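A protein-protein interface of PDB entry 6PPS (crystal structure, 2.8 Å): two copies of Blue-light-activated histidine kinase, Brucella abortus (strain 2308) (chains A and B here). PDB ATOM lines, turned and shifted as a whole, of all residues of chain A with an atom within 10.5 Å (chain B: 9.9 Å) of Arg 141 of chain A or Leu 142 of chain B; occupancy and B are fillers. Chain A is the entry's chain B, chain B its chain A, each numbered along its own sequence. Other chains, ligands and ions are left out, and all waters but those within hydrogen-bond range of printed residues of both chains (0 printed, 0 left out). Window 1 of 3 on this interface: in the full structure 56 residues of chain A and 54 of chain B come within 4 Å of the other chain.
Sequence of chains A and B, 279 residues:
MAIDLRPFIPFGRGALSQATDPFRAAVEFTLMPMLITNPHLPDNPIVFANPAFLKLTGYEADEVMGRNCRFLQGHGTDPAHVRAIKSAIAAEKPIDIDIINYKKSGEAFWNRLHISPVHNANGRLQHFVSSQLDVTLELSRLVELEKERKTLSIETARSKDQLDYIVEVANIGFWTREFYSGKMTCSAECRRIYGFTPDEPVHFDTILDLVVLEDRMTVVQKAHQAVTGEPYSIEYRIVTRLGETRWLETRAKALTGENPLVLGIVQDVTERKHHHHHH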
ATOM      1  N   TRP A 110      36.356 -14.819  -2.966  1.00  0.00           N
ATOM      2  CA  TRP A 110      36.893 -14.140  -1.792  1.00  0.00           C
ATOM      3  C   TRP A 110      36.709 -14.990  -0.543  1.00  0.00           C
ATOM      4  O   TRP A 110      35.596 -15.406  -0.218  1.00  0.00           O
ATOM      5  CB  TRP A 110      36.230 -12.775  -1.605  1.00  0.00           C
ATOM      6  CG  TRP A 110      36.758 -11.723  -2.533  1.00  0.00           C
ATOM      7  CD1 TRP A 110      36.258 -11.383  -3.755  1.00  0.00           C
ATOM      8  CD2 TRP A 110      37.891 -10.877  -2.312  1.00  0.00           C
ATOM      9  NE1 TRP A 110      37.011 -10.376  -4.310  1.00  0.00           N
ATOM     10  CE2 TRP A 110      38.020 -10.047  -3.443  1.00  0.00           C
ATOM     11  CE3 TRP A 110      38.810 -10.741  -1.267  1.00  0.00           C
ATOM     12  CZ2 TRP A 110      39.030  -9.095  -3.559  1.00  0.00           C
ATOM     13  CZ3 TRP A 110      39.812  -9.796  -1.384  1.00  0.00           C
ATOM     14  CH2 TRP A 110      39.913  -8.985  -2.520  1.00  0.00           C
ATOM     15  N   ASP A 134      32.713 -17.780   2.304  1.00  0.00           N
ATOM     16  CA  ASP A 134      32.693 -17.215   0.961  1.00  0.00           C
ATOM     17  C   ASP A 134      31.914 -15.903   0.949  1.00  0.00           C
ATOM     18  O   ASP A 134      30.693 -15.895   1.104  1.00  0.00           O
ATOM     19  CB  ASP A 134      32.084 -18.208  -0.030  1.00  0.00           C
ATOM     20  CG  ASP A 134      32.253 -17.775  -1.472  1.00  0.00           C
ATOM     21  OD1 ASP A 134      33.096 -16.892  -1.735  1.00  0.00           O
ATOM     22  OD2 ASP A 134      31.551 -18.325  -2.346  1.00  0.00           O
ATOM     23  N   VAL A 135      32.630 -14.799   0.771  1.00  0.00           N
ATOM     24  CA  VAL A 135      32.021 -13.474   0.795  1.00  0.00           C
ATOM     25  C   VAL A 135      32.283 -12.716  -0.501  1.00  0.00           C
ATOM     26  O   VAL A 135      32.349 -11.488  -0.512  1.00  0.00           O
ATOM     27  CB  VAL A 135      32.540 -12.643   1.983  1.00  0.00           C
ATOM     28  CG1 VAL A 135      32.027 -13.218   3.296  1.00  0.00           C
ATOM     29  CG2 VAL A 135      34.062 -12.597   1.974  1.00  0.00           C
ATOM     30  N   THR A 136      32.427 -13.459  -1.594  1.00  0.00           N
ATOM     31  CA  THR A 136      32.714 -12.870  -2.897  1.00  0.00           C
ATOM     32  C   THR A 136      31.537 -12.061  -3.422  1.00  0.00           C
ATOM     33  O   THR A 136      31.623 -10.844  -3.574  1.00  0.00           O
ATOM     34  CB  THR A 136      33.070 -13.949  -3.930  1.00  0.00           C
ATOM     35  OG1 THR A 136      34.052 -14.829  -3.378  1.00  0.00           O
ATOM     36  CG2 THR A 136      33.610 -13.314  -5.202  1.00  0.00           C
ATOM     37  N   LEU A 137      30.436 -12.751  -3.696  1.00  0.00           N
ATOM     38  CA  LEU A 137      29.244 -12.111  -4.236  1.00  0.00           C
ATOM     39  C   LEU A 137      28.483 -11.355  -3.154  1.00  0.00           C
ATOM     40  O   LEU A 137      27.524 -10.641  -3.443  1.00  0.00           O
ATOM     41  CB  LEU A 137      28.330 -13.147  -4.898  1.00  0.00           C
ATOM     42  CG  LEU A 137      28.649 -13.564  -6.340  1.00  0.00           C
ATOM     43  CD1 LEU A 137      29.967 -14.324  -6.440  1.00  0.00           C
ATOM     44  CD2 LEU A 137      27.508 -14.387  -6.923  1.00  0.00           C
ATOM     45  N   GLU A 138      28.916 -11.514  -1.907  1.00  0.00           N
ATOM     46  CA  GLU A 138      28.299 -10.812  -0.789  1.00  0.00           C
ATOM     47  C   GLU A 138      28.745  -9.357  -0.726  1.00  0.00           C
ATOM     48  O   GLU A 138      27.916  -8.448  -0.679  1.00  0.00           O
ATOM     49  CB  GLU A 138      28.621 -11.519   0.531  1.00  0.00           C
ATOM     50  CG  GLU A 138      28.479 -10.644   1.773  1.00  0.00           C
ATOM     51  CD  GLU A 138      27.041 -10.254   2.083  1.00  0.00           C
ATOM     52  OE1 GLU A 138      26.838  -9.448   3.016  1.00  0.00           O
ATOM     53  OE2 GLU A 138      26.113 -10.751   1.408  1.00  0.00           O
ATOM     54  N   LEU A 139      30.056  -9.135  -0.725  1.00  0.00           N
ATOM     55  CA  LEU A 139      30.586  -7.778  -0.705  1.00  0.00           C
ATOM     56  C   LEU A 139      30.332  -7.106  -2.048  1.00  0.00           C
ATOM     57  O   LEU A 139      30.103  -5.901  -2.116  1.00  0.00           O
ATOM     58  CB  LEU A 139      32.084  -7.774  -0.363  1.00  0.00           C
ATOM     59  CG  LEU A 139      33.126  -8.336  -1.339  1.00  0.00           C
ATOM     60  CD1 LEU A 139      33.603  -7.281  -2.336  1.00  0.00           C
ATOM     61  CD2 LEU A 139      34.310  -8.918  -0.575  1.00  0.00           C
ATOM     62  N   SER A 140      30.363  -7.901  -3.114  1.00  0.00           N
ATOM     63  CA  SER A 140      30.167  -7.389  -4.465  1.00  0.00           C
ATOM     64  C   SER A 140      28.739  -6.900  -4.678  1.00  0.00           C
ATOM     65  O   SER A 140      28.495  -5.997  -5.478  1.00  0.00           O
ATOM     66  CB  SER A 140      30.514  -8.463  -5.498  1.00  0.00           C
ATOM     67  OG  SER A 140      30.418  -7.953  -6.817  1.00  0.00           O
ATOM     68  N   ARG A 141      27.796  -7.501  -3.960  1.00  0.00           N
ATOM     69  CA  ARG A 141      26.396  -7.111  -4.068  1.00  0.00           C
ATOM     70  C   ARG A 141      26.153  -5.742  -3.441  1.00  0.00           C
ATOM     71  O   ARG A 141      25.384  -4.939  -3.967  1.00  0.00           O
ATOM     72  CB  ARG A 141      25.491  -8.156  -3.409  1.00  0.00           C
ATOM     73  CG  ARG A 141      24.019  -7.772  -3.384  1.00  0.00           C
ATOM     74  CD  ARG A 141      23.463  -7.627  -4.792  1.00  0.00           C
ATOM     75  NE  ARG A 141      22.308  -6.735  -4.836  1.00  0.00           N
ATOM     76  CZ  ARG A 141      21.056  -7.117  -4.609  1.00  0.00           C
ATOM     77  NH1 ARG A 141      20.789  -8.382  -4.315  1.00  0.00           N
ATOM     78  NH2 ARG A 141      20.071  -6.232  -4.671  1.00  0.00           N
ATOM     79  N   LEU A 142      26.821  -5.475  -2.323  1.00  0.00           N
ATOM     80  CA  LEU A 142      26.584  -4.246  -1.577  1.00  0.00           C
ATOM     81  C   LEU A 142      27.421  -3.068  -2.070  1.00  0.00           C
ATOM     82  O   LEU A 142      27.086  -1.915  -1.803  1.00  0.00           O
ATOM     83  CB  LEU A 142      26.840  -4.472  -0.085  1.00  0.00           C
ATOM     84  CG  LEU A 142      25.862  -5.417   0.616  1.00  0.00           C
ATOM     85  CD1 LEU A 142      26.017  -5.325   2.126  1.00  0.00           C
ATOM     86  CD2 LEU A 142      24.429  -5.121   0.198  1.00  0.00           C
ATOM     87  N   VAL A 143      28.507  -3.346  -2.785  1.00  0.00           N
ATOM     88  CA  VAL A 143      29.313  -2.265  -3.344  1.00  0.00           C
ATOM     89  C   VAL A 143      28.686  -1.741  -4.630  1.00  0.00           C
ATOM     90  O   VAL A 143      29.056  -0.673  -5.117  1.00  0.00           O
ATOM     91  CB  VAL A 143      30.765  -2.699  -3.632  1.00  0.00           C
ATOM     92  CG1 VAL A 143      31.478  -3.076  -2.341  1.00  0.00           C
ATOM     93  CG2 VAL A 143      30.797  -3.837  -4.638  1.00  0.00           C
ATOM     94  N   GLU A 144      27.738  -2.495  -5.179  1.00  0.00           N
ATOM     95  CA  GLU A 144      27.033  -2.060  -6.377  1.00  0.00           C
ATOM     96  C   GLU A 144      25.671  -1.478  -6.015  1.00  0.00           C
ATOM     97  O   GLU A 144      25.081  -0.735  -6.798  1.00  0.00           O
ATOM     98  CB  GLU A 144      26.872  -3.216  -7.371  1.00  0.00           C
ATOM     99  CG  GLU A 144      25.656  -4.096  -7.125  1.00  0.00           C
ATOM    100  CD  GLU A 144      25.415  -5.085  -8.251  1.00  0.00           C
ATOM    101  OE1 GLU A 144      26.368  -5.370  -9.007  1.00  0.00           O
ATOM    102  OE2 GLU A 144      24.273  -5.573  -8.383  1.00  0.00           O
ATOM    103  N   LEU A 145      25.177  -1.815  -4.828  1.00  0.00           N
ATOM    104  CA  LEU A 145      23.898  -1.292  -4.360  1.00  0.00           C
ATOM    105  C   LEU A 145      24.049   0.106  -3.777  1.00  0.00           C
ATOM    106  O   LEU A 145      23.080   0.860  -3.694  1.00  0.00           O
ATOM    107  CB  LEU A 145      23.276  -2.221  -3.314  1.00  0.00           C
ATOM    108  CG  LEU A 145      22.535  -3.462  -3.816  1.00  0.00           C
ATOM    109  CD1 LEU A 145      21.694  -4.060  -2.697  1.00  0.00           C
ATOM    110  CD2 LEU A 145      21.677  -3.131  -5.027  1.00  0.00           C
ATOM    111  N   GLU A 146      25.268   0.449  -3.371  1.00  0.00           N
ATOM    112  CA  GLU A 146      25.529   1.756  -2.779  1.00  0.00           C
ATOM    113  C   GLU A 146      26.022   2.754  -3.820  1.00  0.00           C
ATOM    114  O   GLU A 146      26.017   3.962  -3.584  1.00  0.00           O
ATOM    115  CB  GLU A 146      26.541   1.632  -1.638  1.00  0.00           C
ATOM    116  CG  GLU A 146      26.007   0.879  -0.431  1.00  0.00           C
ATOM    117  CD  GLU A 146      24.706   1.465   0.090  1.00  0.00           C
ATOM    118  OE1 GLU A 146      24.758   2.490   0.802  1.00  0.00           O
ATOM    119  OE2 GLU A 146      23.633   0.903  -0.214  1.00  0.00           O
ATOM    120  N   LYS A 147      26.450   2.245  -4.970  1.00  0.00           N
ATOM    121  CA  LYS A 147      26.823   3.104  -6.087  1.00  0.00           C
ATOM    122  C   LYS A 147      25.614   3.360  -6.975  1.00  0.00           C
ATOM    123  O   LYS A 147      25.553   4.353  -7.700  1.00  0.00           O
ATOM    124  CB  LYS A 147      27.958   2.481  -6.901  1.00  0.00           C
ATOM    125  CG  LYS A 147      29.292   2.478  -6.179  1.00  0.00           C
ATOM    126  CD  LYS A 147      29.645   3.877  -5.702  1.00  0.00           C
ATOM    127  CE  LYS A 147      30.873   3.864  -4.811  1.00  0.00           C
ATOM    128  NZ  LYS A 147      31.149   5.209  -4.237  1.00  0.00           N
ATOM    129  N   GLU A 148      24.648   2.452  -6.905  1.00  0.00           N
ATOM    130  CA  GLU A 148      23.430   2.554  -7.693  1.00  0.00           C
ATOM    131  C   GLU A 148      22.460   3.548  -7.063  1.00  0.00           C
ATOM    132  O   GLU A 148      21.726   4.243  -7.764  1.00  0.00           O
ATOM    133  CB  GLU A 148      22.776   1.179  -7.828  1.00  0.00           C
ATOM    134  CG  GLU A 148      21.632   1.108  -8.820  1.00  0.00           C
ATOM    135  CD  GLU A 148      21.381  -0.309  -9.293  1.00  0.00           C
ATOM    136  OE1 GLU A 148      22.367  -1.041  -9.524  1.00  0.00           O
ATOM    137  OE2 GLU A 148      20.201  -0.694  -9.428  1.00  0.00           O
ATOM    138  N   ARG A 149      22.470   3.615  -5.737  1.00  0.00           N
ATOM    139  CA  ARG A 149      21.576   4.511  -5.013  1.00  0.00           C
ATOM    140  C   ARG A 149      21.993   5.968  -5.180  1.00  0.00           C
ATOM    141  O   ARG A 149      21.147   6.859  -5.265  1.00  0.00           O
ATOM    142  CB  ARG A 149      21.538   4.144  -3.528  1.00  0.00           C
ATOM    143  CG  ARG A 149      20.523   4.939  -2.724  1.00  0.00           C
ATOM    144  CD  ARG A 149      20.600   4.595  -1.248  1.00  0.00           C
ATOM    145  NE  ARG A 149      21.920   4.880  -0.695  1.00  0.00           N
ATOM    146  CZ  ARG A 149      22.285   6.062  -0.207  1.00  0.00           C
ATOM    147  NH1 ARG A 149      23.508   6.231   0.276  1.00  0.00           N
ATOM    148  NH2 ARG A 149      21.428   7.073  -0.203  1.00  0.00           N
ATOM    149  N   TRP B 110      17.693 -11.651  13.268  1.00  0.00           N
ATOM    150  CA  TRP B 110      17.364 -12.845  12.502  1.00  0.00           C
ATOM    151  C   TRP B 110      18.391 -13.942  12.739  1.00  0.00           C
ATOM    152  O   TRP B 110      19.559 -13.805  12.376  1.00  0.00           O
ATOM    153  CB  TRP B 110      17.262 -12.522  11.011  1.00  0.00           C
ATOM    154  CG  TRP B 110      15.926 -11.979  10.616  1.00  0.00           C
ATOM    155  CD1 TRP B 110      15.606 -10.673  10.387  1.00  0.00           C
ATOM    156  CD2 TRP B 110      14.724 -12.728  10.414  1.00  0.00           C
ATOM    157  NE1 TRP B 110      14.279 -10.564  10.048  1.00  0.00           N
ATOM    158  CE2 TRP B 110      13.714 -11.813  10.059  1.00  0.00           C
ATOM    159  CE3 TRP B 110      14.402 -14.087  10.497  1.00  0.00           C
ATOM    160  CZ2 TRP B 110      12.408 -12.210   9.786  1.00  0.00           C
ATOM    161  CZ3 TRP B 110      13.105 -14.480  10.227  1.00  0.00           C
ATOM    162  CH2 TRP B 110      12.124 -13.546   9.875  1.00  0.00           C
ATOM    163  N   VAL B 135      21.849 -13.398  10.633  1.00  0.00           N
ATOM    164  CA  VAL B 135      21.601 -12.982   9.258  1.00  0.00           C
ATOM    165  C   VAL B 135      20.627 -11.807   9.183  1.00  0.00           C
ATOM    166  O   VAL B 135      19.837 -11.703   8.245  1.00  0.00           O
ATOM    167  CB  VAL B 135      21.047 -14.147   8.414  1.00  0.00           C
ATOM    168  CG1 VAL B 135      22.122 -15.195   8.186  1.00  0.00           C
ATOM    169  CG2 VAL B 135      19.831 -14.761   9.092  1.00  0.00           C
ATOM    170  N   THR B 136      20.690 -10.924  10.174  1.00  0.00           N
ATOM    171  CA  THR B 136      19.814  -9.758  10.220  1.00  0.00           C
ATOM    172  C   THR B 136      20.054  -8.832   9.029  1.00  0.00           C
ATOM    173  O   THR B 136      19.114  -8.285   8.456  1.00  0.00           O
ATOM    174  CB  THR B 136      20.005  -8.959  11.526  1.00  0.00           C
ATOM    175  OG1 THR B 136      19.781  -9.818  12.651  1.00  0.00           O
ATOM    176  CG2 THR B 136      19.036  -7.785  11.589  1.00  0.00           C
ATOM    177  N   LEU B 137      21.318  -8.672   8.651  1.00  0.00           N
ATOM    178  CA  LEU B 137      21.680  -7.755   7.577  1.00  0.00           C
ATOM    179  C   LEU B 137      21.317  -8.294   6.195  1.00  0.00           C
ATOM    180  O   LEU B 137      21.425  -7.579   5.200  1.00  0.00           O
ATOM    181  CB  LEU B 137      23.176  -7.436   7.632  1.00  0.00           C
ATOM    182  CG  LEU B 137      23.655  -6.717   8.895  1.00  0.00           C
ATOM    183  CD1 LEU B 137      25.091  -6.240   8.730  1.00  0.00           C
ATOM    184  CD2 LEU B 137      22.735  -5.556   9.242  1.00  0.00           C
ATOM    185  N   GLU B 138      20.889  -9.551   6.134  1.00  0.00           N
ATOM    186  CA  GLU B 138      20.474 -10.148   4.869  1.00  0.00           C
ATOM    187  C   GLU B 138      18.955 -10.154   4.713  1.00  0.00           C
ATOM    188  O   GLU B 138      18.427  -9.720   3.689  1.00  0.00           O
ATOM    189  CB  GLU B 138      21.011 -11.575   4.740  1.00  0.00           C
ATOM    190  CG  GLU B 138      20.477 -12.317   3.521  1.00  0.00           C
ATOM    191  CD  GLU B 138      20.964 -13.752   3.440  1.00  0.00           C
ATOM    192  OE1 GLU B 138      22.016 -14.060   4.036  1.00  0.00           O
ATOM    193  OE2 GLU B 138      20.289 -14.572   2.781  1.00  0.00           O
ATOM    194  N   LEU B 139      18.258 -10.645   5.732  1.00  0.00           N
ATOM    195  CA  LEU B 139      16.809 -10.802   5.657  1.00  0.00           C
ATOM    196  C   LEU B 139      16.042  -9.541   6.043  1.00  0.00           C
ATOM    197  O   LEU B 139      14.835  -9.453   5.816  1.00  0.00           O
ATOM    198  CB  LEU B 139      16.354 -11.959   6.548  1.00  0.00           C
ATOM    199  CG  LEU B 139      16.856 -13.357   6.193  1.00  0.00           C
ATOM    200  CD1 LEU B 139      16.079 -14.396   6.982  1.00  0.00           C
ATOM    201  CD2 LEU B 139      16.746 -13.617   4.698  1.00  0.00           C
ATOM    202  N   SER B 140      16.732  -8.568   6.626  1.00  0.00           N
ATOM    203  CA  SER B 140      16.062  -7.361   7.096  1.00  0.00           C
ATOM    204  C   SER B 140      16.625  -6.092   6.462  1.00  0.00           C
ATOM    205  O   SER B 140      15.884  -5.145   6.195  1.00  0.00           O
ATOM    206  CB  SER B 140      16.151  -7.263   8.622  1.00  0.00           C
ATOM    207  OG  SER B 140      15.389  -6.174   9.112  1.00  0.00           O
ATOM    208  N   ARG B 141      17.931  -6.071   6.216  1.00  0.00           N
ATOM    209  CA  ARG B 141      18.573  -4.883   5.662  1.00  0.00           C
ATOM    210  C   ARG B 141      18.606  -4.900   4.135  1.00  0.00           C
ATOM    211  O   ARG B 141      18.212  -3.929   3.492  1.00  0.00           O
ATOM    212  CB  ARG B 141      19.996  -4.736   6.207  1.00  0.00           C
ATOM    213  CG  ARG B 141      20.736  -3.530   5.653  1.00  0.00           C
ATOM    214  CD  ARG B 141      22.156  -3.440   6.191  1.00  0.00           C
ATOM    215  NE  ARG B 141      22.906  -2.361   5.552  1.00  0.00           N
ATOM    216  CZ  ARG B 141      24.175  -2.071   5.818  1.00  0.00           C
ATOM    217  NH1 ARG B 141      24.847  -2.777   6.715  1.00  0.00           N
ATOM    218  NH2 ARG B 141      24.773  -1.071   5.183  1.00  0.00           N
ATOM    219  N   LEU B 142      19.081  -5.999   3.559  1.00  0.00           N
ATOM    220  CA  LEU B 142      19.193  -6.108   2.107  1.00  0.00           C
ATOM    221  C   LEU B 142      17.815  -6.130   1.454  1.00  0.00           C
ATOM    222  O   LEU B 142      17.623  -5.573   0.374  1.00  0.00           O
ATOM    223  CB  LEU B 142      19.986  -7.363   1.725  1.00  0.00           C
ATOM    224  CG  LEU B 142      20.594  -7.455   0.320  1.00  0.00           C
ATOM    225  CD1 LEU B 142      21.777  -8.407   0.332  1.00  0.00           C
ATOM    226  CD2 LEU B 142      19.575  -7.903  -0.722  1.00  0.00           C
ATOM    227  N   VAL B 143      16.863  -6.776   2.119  1.00  0.00           N
ATOM    228  CA  VAL B 143      15.514  -6.927   1.587  1.00  0.00           C
ATOM    229  C   VAL B 143      14.831  -5.576   1.397  1.00  0.00           C
ATOM    230  O   VAL B 143      14.148  -5.353   0.395  1.00  0.00           O
ATOM    231  CB  VAL B 143      14.651  -7.818   2.505  1.00  0.00           C
ATOM    232  CG1 VAL B 143      13.220  -7.891   1.994  1.00  0.00           C
ATOM    233  CG2 VAL B 143      15.255  -9.209   2.603  1.00  0.00           C
ATOM    234  N   GLU B 144      15.025  -4.669   2.349  1.00  0.00           N
ATOM    235  CA  GLU B 144      14.414  -3.348   2.258  1.00  0.00           C
ATOM    236  C   GLU B 144      15.173  -2.451   1.280  1.00  0.00           C
ATOM    237  O   GLU B 144      14.591  -1.546   0.686  1.00  0.00           O
ATOM    238  CB  GLU B 144      14.335  -2.684   3.636  1.00  0.00           C
ATOM    239  CG  GLU B 144      15.668  -2.232   4.204  1.00  0.00           C
ATOM    240  CD  GLU B 144      15.518  -1.461   5.500  1.00  0.00           C
ATOM    241  OE1 GLU B 144      14.384  -1.381   6.018  1.00  0.00           O
ATOM    242  OE2 GLU B 144      16.533  -0.932   6.000  1.00  0.00           O
ATOM    243  N   LEU B 145      16.466  -2.710   1.108  1.00  0.00           N
ATOM    244  CA  LEU B 145      17.274  -1.938   0.168  1.00  0.00           C
ATOM    245  C   LEU B 145      16.949  -2.324  -1.270  1.00  0.00           C
ATOM    246  O   LEU B 145      17.278  -1.601  -2.208  1.00  0.00           O
ATOM    247  CB  LEU B 145      18.767  -2.132   0.441  1.00  0.00           C
ATOM    248  CG  LEU B 145      19.326  -1.502   1.719  1.00  0.00           C
ATOM    249  CD1 LEU B 145      20.833  -1.701   1.799  1.00  0.00           C
ATOM    250  CD2 LEU B 145      18.967  -0.024   1.802  1.00  0.00           C
ATOM    251  N   GLU B 146      16.303  -3.475  -1.433  1.00  0.00           N
ATOM    252  CA  GLU B 146      15.873  -3.935  -2.746  1.00  0.00           C
ATOM    253  C   GLU B 146      14.529  -3.311  -3.107  1.00  0.00           C
ATOM    254  O   GLU B 146      14.260  -3.023  -4.273  1.00  0.00           O
ATOM    255  CB  GLU B 146      15.783  -5.463  -2.775  1.00  0.00           C
ATOM    256  CG  GLU B 146      15.542  -6.062  -4.155  1.00  0.00           C
ATOM    257  CD  GLU B 146      16.778  -6.034  -5.036  1.00  0.00           C
ATOM    258  OE1 GLU B 146      17.849  -5.605  -4.557  1.00  0.00           O
ATOM    259  OE2 GLU B 146      16.680  -6.449  -6.211  1.00  0.00           O
ATOM    260  N   LYS B 147      13.690  -3.104  -2.097  1.00  0.00           N
ATOM    261  CA  LYS B 147      12.387  -2.479  -2.293  1.00  0.00           C
ATOM    262  C   LYS B 147      12.504  -0.957  -2.295  1.00  0.00           C
ATOM    263  O   LYS B 147      11.643  -0.259  -2.829  1.00  0.00           O
ATOM    264  CB  LYS B 147      11.404  -2.933  -1.212  1.00  0.00           C
ATOM    265  CG  LYS B 147      11.037  -4.407  -1.283  1.00  0.00           C
ATOM    266  CD  LYS B 147      10.341  -4.736  -2.595  1.00  0.00           C
ATOM    267  CE  LYS B 147       9.942  -6.203  -2.662  1.00  0.00           C
ATOM    268  NZ  LYS B 147       9.250  -6.529  -3.939  1.00  0.00           N
ATOM    269  N   GLU B 148      13.574  -0.451  -1.689  1.00  0.00           N
ATOM    270  CA  GLU B 148      13.850   0.982  -1.689  1.00  0.00           C
ATOM    271  C   GLU B 148      14.406   1.414  -3.040  1.00  0.00           C
ATOM    272  O   GLU B 148      14.027   2.455  -3.576  1.00  0.00           O
ATOM    273  CB  GLU B 148      14.829   1.344  -0.572  1.00  0.00           C
ATOM    274  CG  GLU B 148      15.277   2.796  -0.579  1.00  0.00           C
ATOM    275  CD  GLU B 148      16.142   3.144   0.618  1.00  0.00           C
ATOM    276  OE1 GLU B 148      17.383   3.087   0.495  1.00  0.00           O
ATOM    277  OE2 GLU B 148      15.578   3.473   1.683  1.00  0.00           O
ATOM    278  N   ARG B 149      15.309   0.602  -3.580  1.00  0.00           N
ATOM    279  CA  ARG B 149      15.884   0.852  -4.897  1.00  0.00           C
ATOM    280  C   ARG B 149      14.816   0.760  -5.981  1.00  0.00           C
ATOM    281  O   ARG B 149      14.790   1.565  -6.912  1.00  0.00           O
ATOM    282  CB  ARG B 149      17.010  -0.143  -5.185  1.00  0.00           C
ATOM    283  CG  ARG B 149      17.628   0.001  -6.565  1.00  0.00           C
ATOM    284  CD  ARG B 149      18.020  -1.354  -7.129  1.00  0.00           C
ATOM    285  NE  ARG B 149      16.853  -2.204  -7.351  1.00  0.00           N
ATOM    286  CZ  ARG B 149      16.165  -2.245  -8.488  1.00  0.00           C
ATOM    287  NH1 ARG B 149      16.526  -1.485  -9.512  1.00  0.00           N
ATOM    288  NH2 ARG B 149      15.114  -3.047  -8.601  1.00  0.00           N
ATOM    289  N   LYS B 150      13.937  -0.228  -5.848  1.00  0.00           N
ATOM    290  CA  LYS B 150      12.852  -0.434  -6.801  1.00  0.00           C
ATOM    291  C   LYS B 150      11.874   0.739  -6.786  1.00  0.00           C
ATOM    292  O   LYS B 150      11.281   1.078  -7.810  1.00  0.00           O
ATOM    293  CB  LYS B 150      12.116  -1.740  -6.496  1.00  0.00           C
ATOM    294  CG  LYS B 150      11.049  -2.107  -7.512  1.00  0.00           C
ATOM    295  CD  LYS B 150      10.215  -3.281  -7.031  1.00  0.00           C
ATOM    296  CE  LYS B 150       9.493  -2.943  -5.737  1.00  0.00           C
ATOM    297  NZ  LYS B 150       8.613  -1.750  -5.892  1.00  0.00           N
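Arg 141 of chain A touches Leu 142 of chain B, but with the chains exchanged Leu 142 of chain A does not touch Arg 141 of chain B (5.3 Å).
Arg 141 of chain A touches Glu 146 of chain B, but with the chains exchanged Glu 146 of chain A does not touch Arg 141 of chain B (5.6 Å).
Glu 148 of chain A touches Arg 149 of chain B, and with the chains exchanged Arg 149 of chain A touches Glu 148 of chain B.
Of the 4 pairs that touch across the chains among the printed residues, 2 have their exchanged pair printed and touching as well.
Arg 141 of chain A touches just these residues of chain B: Leu 142 and Glu 146.
Leu 142 of chain B touches just one residue of chain A: Arg 141 (3.8 Å).
No residue of chain A comes within 4 Å of Val 143 of chain B.
Glu 146 of chain B touches just one residue of chain A: Arg 141.
Printed residues of chain B within 4 Å of Glu 148 of chain A: Arg 149 (3.2 Å).
Of the printed residues of chain B, Arg 149 of chain A touches Glu 148.
Printed residues of chain A within 4 Å of Glu 148 of chain B: Arg 149 (3.96 Å).
Trp 110 of chain A touches none of the printed residues of chain B.
The nearest residue of chain B that does not touch Arg 141 of chain A is Arg 149 of chain B (5.8 Å).
Among the printed residues, merely in contact across the chains: Arg 141 of chain A with Leu 142 of chain B (3.8 Å) and Arg 149 of chain A with Glu 148 of chain B (3.96 Å).
The backbone NH (N) of Leu 142 of chain B sits at hydrogen-bond distance from the backbone carbonyl oxygen (O) of Leu 137 of chain B (3.3 Å).
The side-chain carboxylate (OE1) of Glu 146 of chain A is in salt-bridge range of the guanidinium group (NH1) of Arg 149 of chain A, 3.98 Å away.
Of the 17 printed residues of chain A, 3 touch a printed residue of chain B.
Printed residues of chain A that touch a printed residue of chain B: Arg 141, Glu 148 and Arg 149.
Of the 17 printed residues of chain B, 4 touch a printed residue of chain A.
Printed residues of chain B that touch a printed residue of chain A: Leu 142, Glu 146, Glu 148 and Arg 149.
Among the printed residues, 4 pairs touch across the chains.
Among the printed residues, Asp or Glu carboxylates within 4 Å of a Lys or Arg side-chain nitrogen of the other chain: Arg 141 of chain A with Glu 146 of chain B and Glu 148 of chain A with Arg 149 of chain B.
The guanidinium group (NH1) of Arg 149 of chain B is in salt-bridge range of the side-chain carboxylate (OE2) of Glu 148 of chain A (3.8 Å).
The side-chain carboxylate (OE2) of Glu 146 of chain B is in salt-bridge range of the guanidinium group (NH2) of Arg 141 of chain A (3.7 Å).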
